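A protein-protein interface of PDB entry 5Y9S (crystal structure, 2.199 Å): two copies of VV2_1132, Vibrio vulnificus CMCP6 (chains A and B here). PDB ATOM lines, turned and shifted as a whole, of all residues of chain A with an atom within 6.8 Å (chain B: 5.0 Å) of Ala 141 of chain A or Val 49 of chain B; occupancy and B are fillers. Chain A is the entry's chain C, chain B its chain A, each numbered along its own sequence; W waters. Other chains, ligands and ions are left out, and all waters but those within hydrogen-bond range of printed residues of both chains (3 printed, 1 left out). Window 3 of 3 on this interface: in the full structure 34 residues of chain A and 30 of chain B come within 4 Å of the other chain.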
ATOM      1  N   LYS A  87       5.077   1.516  15.427  1.00  0.00           N
ATOM      2  CA  LYS A  87       4.163   2.614  15.709  1.00  0.00           C
ATOM      3  C   LYS A  87       4.848   3.698  16.526  1.00  0.00           C
ATOM      4  O   LYS A  87       4.688   4.892  16.246  1.00  0.00           O
ATOM      5  CB  LYS A  87       2.937   2.086  16.455  1.00  0.00           C
ATOM      6  CG  LYS A  87       1.843   3.118  16.651  1.00  0.00           C
ATOM      7  CD  LYS A  87       0.995   3.222  15.398  1.00  0.00           C
ATOM      8  CE  LYS A  87      -0.429   3.711  15.676  1.00  0.00           C
ATOM      9  NZ  LYS A  87      -1.234   3.747  14.401  1.00  0.00           N
ATOM     10  N   LEU A 137      -7.659  13.984   3.281  1.00  0.00           N
ATOM     11  CA  LEU A 137      -7.569  12.524   3.358  1.00  0.00           C
ATOM     12  C   LEU A 137      -8.902  11.832   3.599  1.00  0.00           C
ATOM     13  O   LEU A 137      -8.947  10.595   3.533  1.00  0.00           O
ATOM     14  CB  LEU A 137      -6.606  12.098   4.476  1.00  0.00           C
ATOM     15  CG  LEU A 137      -5.135  12.444   4.269  1.00  0.00           C
ATOM     16  CD1 LEU A 137      -4.328  11.758   5.306  1.00  0.00           C
ATOM     17  CD2 LEU A 137      -4.692  12.005   2.875  1.00  0.00           C
ATOM     18  N   GLY A 138      -9.974  12.581   3.873  1.00  0.00           N
ATOM     19  CA  GLY A 138     -11.252  11.994   4.229  1.00  0.00           C
ATOM     20  C   GLY A 138     -11.500  12.204   5.702  1.00  0.00           C
ATOM     21  O   GLY A 138     -10.547  12.142   6.490  1.00  0.00           O
ATOM     22  N   ILE A 139     -12.753  12.440   6.104  1.00  0.00           N
ATOM     23  CA  ILE A 139     -12.978  12.896   7.475  1.00  0.00           C
ATOM     24  C   ILE A 139     -12.578  11.813   8.473  1.00  0.00           C
ATOM     25  O   ILE A 139     -11.997  12.109   9.522  1.00  0.00           O
ATOM     26  CB  ILE A 139     -14.434  13.378   7.670  1.00  0.00           C
ATOM     27  CG1 ILE A 139     -14.558  14.226   8.933  1.00  0.00           C
ATOM     28  CG2 ILE A 139     -15.403  12.225   7.803  1.00  0.00           C
ATOM     29  CD1 ILE A 139     -13.476  15.256   9.087  1.00  0.00           C
ATOM     30  N   ASP A 140     -12.865  10.542   8.166  1.00  0.00           N
ATOM     31  CA  ASP A 140     -12.495   9.464   9.092  1.00  0.00           C
ATOM     32  C   ASP A 140     -10.982   9.313   9.208  1.00  0.00           C
ATOM     33  O   ASP A 140     -10.458   9.095  10.301  1.00  0.00           O
ATOM     34  CB  ASP A 140     -13.107   8.138   8.654  1.00  0.00           C
ATOM     35  CG  ASP A 140     -14.600   8.088   8.879  1.00  0.00           C
ATOM     36  OD1 ASP A 140     -15.081   8.733   9.834  1.00  0.00           O
ATOM     37  OD2 ASP A 140     -15.284   7.393   8.104  1.00  0.00           O
ATOM     38  N   ALA A 141     -10.269   9.396   8.088  1.00  0.00           N
ATOM     39  CA  ALA A 141      -8.811   9.326   8.130  1.00  0.00           C
ATOM     40  C   ALA A 141      -8.234  10.395   9.050  1.00  0.00           C
ATOM     41  O   ALA A 141      -7.391  10.101   9.902  1.00  0.00           O
ATOM     42  CB  ALA A 141      -8.240   9.461   6.717  1.00  0.00           C
ATOM     43  N   HIS A 142      -8.693  11.644   8.913  1.00  0.00           N
ATOM     44  CA  HIS A 142      -8.135  12.704   9.754  1.00  0.00           C
ATOM     45  C   HIS A 142      -8.467  12.478  11.227  1.00  0.00           C
ATOM     46  O   HIS A 142      -7.604  12.658  12.095  1.00  0.00           O
ATOM     47  CB  HIS A 142      -8.601  14.083   9.259  1.00  0.00           C
ATOM     48  CG  HIS A 142      -7.933  14.506   7.984  1.00  0.00           C
ATOM     49  ND1 HIS A 142      -6.562  14.647   7.873  1.00  0.00           N
ATOM     50  CD2 HIS A 142      -8.433  14.730   6.744  1.00  0.00           C
ATOM     51  CE1 HIS A 142      -6.254  14.986   6.633  1.00  0.00           C
ATOM     52  NE2 HIS A 142      -7.371  15.035   5.926  1.00  0.00           N
ATOM     53  N   PHE A 143      -9.686  12.036  11.536  1.00  0.00           N
ATOM     54  CA  PHE A 143     -10.023  11.801  12.946  1.00  0.00           C
ATOM     55  C   PHE A 143      -9.202  10.663  13.538  1.00  0.00           C
ATOM     56  O   PHE A 143      -8.819  10.709  14.719  1.00  0.00           O
ATOM     57  CB  PHE A 143     -11.515  11.524  13.109  1.00  0.00           C
ATOM     58  CG  PHE A 143     -12.317  12.760  13.314  1.00  0.00           C
ATOM     59  CD1 PHE A 143     -12.086  13.569  14.407  1.00  0.00           C
ATOM     60  CD2 PHE A 143     -13.278  13.135  12.396  1.00  0.00           C
ATOM     61  CE1 PHE A 143     -12.810  14.730  14.593  1.00  0.00           C
ATOM     62  CE2 PHE A 143     -14.003  14.300  12.566  1.00  0.00           C
ATOM     63  CZ  PHE A 143     -13.766  15.100  13.669  1.00  0.00           C
ATOM     64  N   GLN A 144      -8.891   9.660  12.731  1.00  0.00           N
ATOM     65  CA  GLN A 144      -8.034   8.585  13.208  1.00  0.00           C
ATOM     66  C   GLN A 144      -6.649   9.125  13.549  1.00  0.00           C
ATOM     67  O   GLN A 144      -6.077   8.787  14.596  1.00  0.00           O
ATOM     68  CB  GLN A 144      -7.993   7.504  12.138  1.00  0.00           C
ATOM     69  CG  GLN A 144      -7.362   6.190  12.467  1.00  0.00           C
ATOM     70  CD  GLN A 144      -7.182   5.369  11.190  1.00  0.00           C
ATOM     71  OE1 GLN A 144      -6.074   4.925  10.865  1.00  0.00           O
ATOM     72  NE2 GLN A 144      -8.270   5.216  10.430  1.00  0.00           N
ATOM     73  N   MET A 145      -6.131  10.041  12.713  1.00  0.00           N
ATOM     74  CA  MET A 145      -4.842  10.677  12.995  1.00  0.00           C
ATOM     75  C   MET A 145      -4.919  11.500  14.277  1.00  0.00           C
ATOM     76  O   MET A 145      -3.987  11.482  15.099  1.00  0.00           O
ATOM     77  CB  MET A 145      -4.414  11.535  11.807  1.00  0.00           C
ATOM     78  CG  MET A 145      -4.194  10.697  10.536  1.00  0.00           C
ATOM     79  SD  MET A 145      -2.939  11.334   9.431  1.00  0.00           S
ATOM     80  CE  MET A 145      -3.809  12.564   8.511  1.00  0.00           C
ATOM     81  N   LEU A 146      -6.046  12.182  14.492  1.00  0.00           N
ATOM     82  CA  LEU A 146      -6.233  12.943  15.728  1.00  0.00           C
ATOM     83  C   LEU A 146      -6.156  12.019  16.925  1.00  0.00           C
ATOM     84  O   LEU A 146      -5.475  12.319  17.914  1.00  0.00           O
ATOM     85  CB  LEU A 146      -7.583  13.675  15.723  1.00  0.00           C
ATOM     86  CG  LEU A 146      -7.843  14.776  16.758  1.00  0.00           C
ATOM     87  CD1 LEU A 146      -6.917  15.971  16.530  1.00  0.00           C
ATOM     88  CD2 LEU A 146      -9.299  15.222  16.670  1.00  0.00           C
ATOM     89  N   ASP A 148      -4.821   8.998  17.060  1.00  0.00           N
ATOM     90  CA  ASP A 148      -3.458   8.471  17.166  1.00  0.00           C
ATOM     91  C   ASP A 148      -2.441   9.515  17.602  1.00  0.00           C
ATOM     92  O   ASP A 148      -1.294   9.145  17.871  1.00  0.00           O
ATOM     93  CB  ASP A 148      -2.988   7.892  15.834  1.00  0.00           C
ATOM     94  CG  ASP A 148      -3.505   6.502  15.583  1.00  0.00           C
ATOM     95  OD1 ASP A 148      -3.340   6.021  14.436  1.00  0.00           O
ATOM     96  OD2 ASP A 148      -4.066   5.890  16.524  1.00  0.00           O
ATOM     97  N   SER A 150      -1.020  11.676  15.662  1.00  0.00           N
ATOM     98  CA  SER A 150      -0.162  12.196  14.608  1.00  0.00           C
ATOM     99  C   SER A 150      -0.647  13.560  14.118  1.00  0.00           C
ATOM    100  O   SER A 150       0.023  14.188  13.295  1.00  0.00           O
ATOM    101  CB  SER A 150      -0.053  11.188  13.458  1.00  0.00           C
ATOM    102  OG  SER A 150      -1.311  10.670  13.095  1.00  0.00           O
ATOM    103  N   GLN B  45      -2.831   4.742   1.090  1.00  0.00           N
ATOM    104  CA  GLN B  45      -3.213   5.792   2.030  1.00  0.00           C
ATOM    105  C   GLN B  45      -3.481   5.228   3.423  1.00  0.00           C
ATOM    106  O   GLN B  45      -3.140   5.858   4.439  1.00  0.00           O
ATOM    107  CB  GLN B  45      -4.451   6.510   1.557  1.00  0.00           C
ATOM    108  CG  GLN B  45      -5.123   7.196   2.700  1.00  0.00           C
ATOM    109  CD  GLN B  45      -6.065   8.294   2.259  1.00  0.00           C
ATOM    110  OE1 GLN B  45      -5.839   8.992   1.249  1.00  0.00           O
ATOM    111  NE2 GLN B  45      -7.166   8.433   3.013  1.00  0.00           N
ATOM    112  N   ALA B  46      -4.150   4.072   3.508  1.00  0.00           N
ATOM    113  CA  ALA B  46      -4.426   3.548   4.848  1.00  0.00           C
ATOM    114  C   ALA B  46      -3.127   3.288   5.597  1.00  0.00           C
ATOM    115  O   ALA B  46      -3.042   3.542   6.801  1.00  0.00           O
ATOM    116  CB  ALA B  46      -5.288   2.283   4.784  1.00  0.00           C
ATOM    117  N   LEU B  47      -2.080   2.820   4.892  1.00  0.00           N
ATOM    118  CA  LEU B  47      -0.806   2.578   5.567  1.00  0.00           C
ATOM    119  C   LEU B  47      -0.181   3.890   6.045  1.00  0.00           C
ATOM    120  O   LEU B  47       0.275   3.984   7.191  1.00  0.00           O
ATOM    121  CB  LEU B  47       0.137   1.821   4.640  1.00  0.00           C
ATOM    122  CG  LEU B  47       1.614   1.706   5.055  1.00  0.00           C
ATOM    123  CD1 LEU B  47       1.781   0.905   6.352  1.00  0.00           C
ATOM    124  CD2 LEU B  47       2.437   1.086   3.929  1.00  0.00           C
ATOM    125  N   GLU B  48      -0.207   4.931   5.195  1.00  0.00           N
ATOM    126  CA  GLU B  48       0.350   6.235   5.567  1.00  0.00           C
ATOM    127  C   GLU B  48      -0.428   6.871   6.719  1.00  0.00           C
ATOM    128  O   GLU B  48       0.179   7.359   7.688  1.00  0.00           O
ATOM    129  CB  GLU B  48       0.380   7.146   4.335  1.00  0.00           C
ATOM    130  CG  GLU B  48       1.378   6.651   3.276  1.00  0.00           C
ATOM    131  CD  GLU B  48       1.442   7.534   2.026  1.00  0.00           C
ATOM    132  OE1 GLU B  48       2.579   7.880   1.630  1.00  0.00           O
ATOM    133  OE2 GLU B  48       0.390   7.844   1.413  1.00  0.00           O
ATOM    134  N   VAL B  49      -1.765   6.836   6.668  1.00  0.00           N
ATOM    135  CA  VAL B  49      -2.569   7.292   7.815  1.00  0.00           C
ATOM    136  C   VAL B  49      -2.161   6.549   9.084  1.00  0.00           C
ATOM    137  O   VAL B  49      -1.982   7.150  10.141  1.00  0.00           O
ATOM    138  CB  VAL B  49      -4.074   7.096   7.552  1.00  0.00           C
ATOM    139  CG1 VAL B  49      -4.848   7.289   8.870  1.00  0.00           C
ATOM    140  CG2 VAL B  49      -4.576   8.041   6.504  1.00  0.00           C
ATOM    141  N   TRP B  50      -2.052   5.214   9.007  1.00  0.00           N
ATOM    142  CA  TRP B  50      -1.742   4.415  10.201  1.00  0.00           C
ATOM    143  C   TRP B  50      -0.391   4.798  10.784  1.00  0.00           C
ATOM    144  O   TRP B  50      -0.247   4.979  12.002  1.00  0.00           O
ATOM    145  CB  TRP B  50      -1.750   2.915   9.852  1.00  0.00           C
ATOM    146  CG  TRP B  50      -1.437   2.008  11.019  1.00  0.00           C
ATOM    147  CD1 TRP B  50      -2.330   1.471  11.902  1.00  0.00           C
ATOM    148  CD2 TRP B  50      -0.134   1.528  11.427  1.00  0.00           C
ATOM    149  NE1 TRP B  50      -1.663   0.700  12.838  1.00  0.00           N
ATOM    150  CE2 TRP B  50      -0.323   0.714  12.565  1.00  0.00           C
ATOM    151  CE3 TRP B  50       1.158   1.687  10.927  1.00  0.00           C
ATOM    152  CZ2 TRP B  50       0.738   0.071  13.214  1.00  0.00           C
ATOM    153  CZ3 TRP B  50       2.216   1.054  11.586  1.00  0.00           C
ATOM    154  CH2 TRP B  50       1.995   0.266  12.716  1.00  0.00           C
ATOM    155  N   ILE B  51       0.628   4.892   9.925  1.00  0.00           N
ATOM    156  CA  ILE B  51       1.947   5.225  10.438  1.00  0.00           C
ATOM    157  C   ILE B  51       2.025   6.695  10.843  1.00  0.00           C
ATOM    158  O   ILE B  51       2.750   7.050  11.777  1.00  0.00           O
ATOM    159  CB  ILE B  51       3.016   4.844   9.405  1.00  0.00           C
ATOM    160  CG1 ILE B  51       4.374   4.966  10.025  1.00  0.00           C
ATOM    161  CG2 ILE B  51       2.946   5.724   8.192  1.00  0.00           C
ATOM    162  CD1 ILE B  51       5.200   3.801   9.705  1.00  0.00           C
ATOM    163  N   GLY B  52       1.281   7.570  10.185  1.00  0.00           N
ATOM    164  CA  GLY B  52       1.218   8.946  10.615  1.00  0.00           C
ATOM    165  C   GLY B  52       1.943   9.935   9.725  1.00  0.00           C
ATOM    166  O   GLY B  52       1.819  11.135   9.956  1.00  0.00           O
HETATM  167  O   HOH W   1      -3.039   1.577  15.404  1.00  0.00           O
HETATM  168  O   HOH W   2      -5.377   3.634   8.405  1.00  0.00           O
HETATM  169  O   HOH W   3       2.716   5.857  14.056  1.00  0.00           O
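The side-chain amino group (NZ) of Lys 87 of chain A is in salt-bridge range of the side-chain carboxylate (OD1) of Asp 148 of chain A, 3.1 Å away. A ring nitrogen (NE2) of His 142 of chain A is in hydrogen-bond range of the backbone NH (N) of Leu 137 of chain A, 2.9 Å away. N of Ser 150 of chain A is in hydrogen-bond range of O of Met 145 of chain A, at 3.0 Å.
No position is printed for both chains. Of the 8 pairs that touch across the chains among the printed residues, none has its exchanged pair printed and touching as well.
Printed residues of chain B within 4 Å of Ala 141 of chain A: Gln 45 (3.99 Å) and Val 49 (3.9 Å). Of chain A, only Leu 137, Ala 141, Gln 144 and Met 145 come within 4 Å of Val 49 of chain B. Printed residues of chain B within 4 Å of Gln 144 of chain A: Val 49 (3.3 Å). Printed residues of chain B within 4 Å of Met 145 of chain A: Val 49 (3.8 Å). Printed residues of chain B within 4 Å of Lys 87 of chain A: Trp 50 (2.9 Å). Of the printed residues of chain A, Gly 52 of chain B touches Ser 150 (3.8 Å). Of the printed residues of chain B, Leu 137 of chain A touches Gln 45 and Val 49. Asp 140 of chain A touches none of the printed residues of chain B. The nearest printed residue of chain B that does not touch Ala 141 of chain A is Ala 46 of chain B (7.3 Å).
Water W3 bridges O of Ile 51 of chain B and O of Lys 87 of chain A. Water W2 bridges O of Ala 46 of chain B (2.8 Å) and OE1 of Gln 144 of chain A (2.9 Å). Water W1 bridges NZ of Lys 87 of chain A (3.0 Å) and NE1 of Trp 50 of chain B (3.0 Å).
Printed residues of chain B that touch a printed residue of chain A: Gln 45, Val 49, Trp 50 and Gly 52. Hydrophobic or aromatic side chains of chain B within 4 Å of the printed part of chain A: Val 49 and Trp 50. Hydrophobic or aromatic side chains of chain A that line the printed part of chain B: Leu 137, Ala 141 and Met 145. Along chain A the printed residues that touch a printed residue of chain B span positions 87 to 150. Among the printed residues, 8 pairs touch across the chains.
NE2 of Gln 45 of chain B lies within hydrogen-bond range of O of Leu 137 of chain A (2.8 Å). The backbone carbonyl oxygen (O) of Trp 50 of chain B sits at hydrogen-bond distance from the side-chain amino group (NZ) of Lys 87 of chain A (2.9 Å).
Among the printed residues, pairs that only touch across the chains: Leu 137 of chain A with Val 49 of chain B, Ala 141 of chain A with Gln 45 of chain B, Ala 141 of chain A with Val 49 of chain B, Gln 144 of chain A with Val 49 of chain B, Met 145 of chain A with Val 49 of chain B and Ser 150 of chain A with Gly 52 of chain B.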
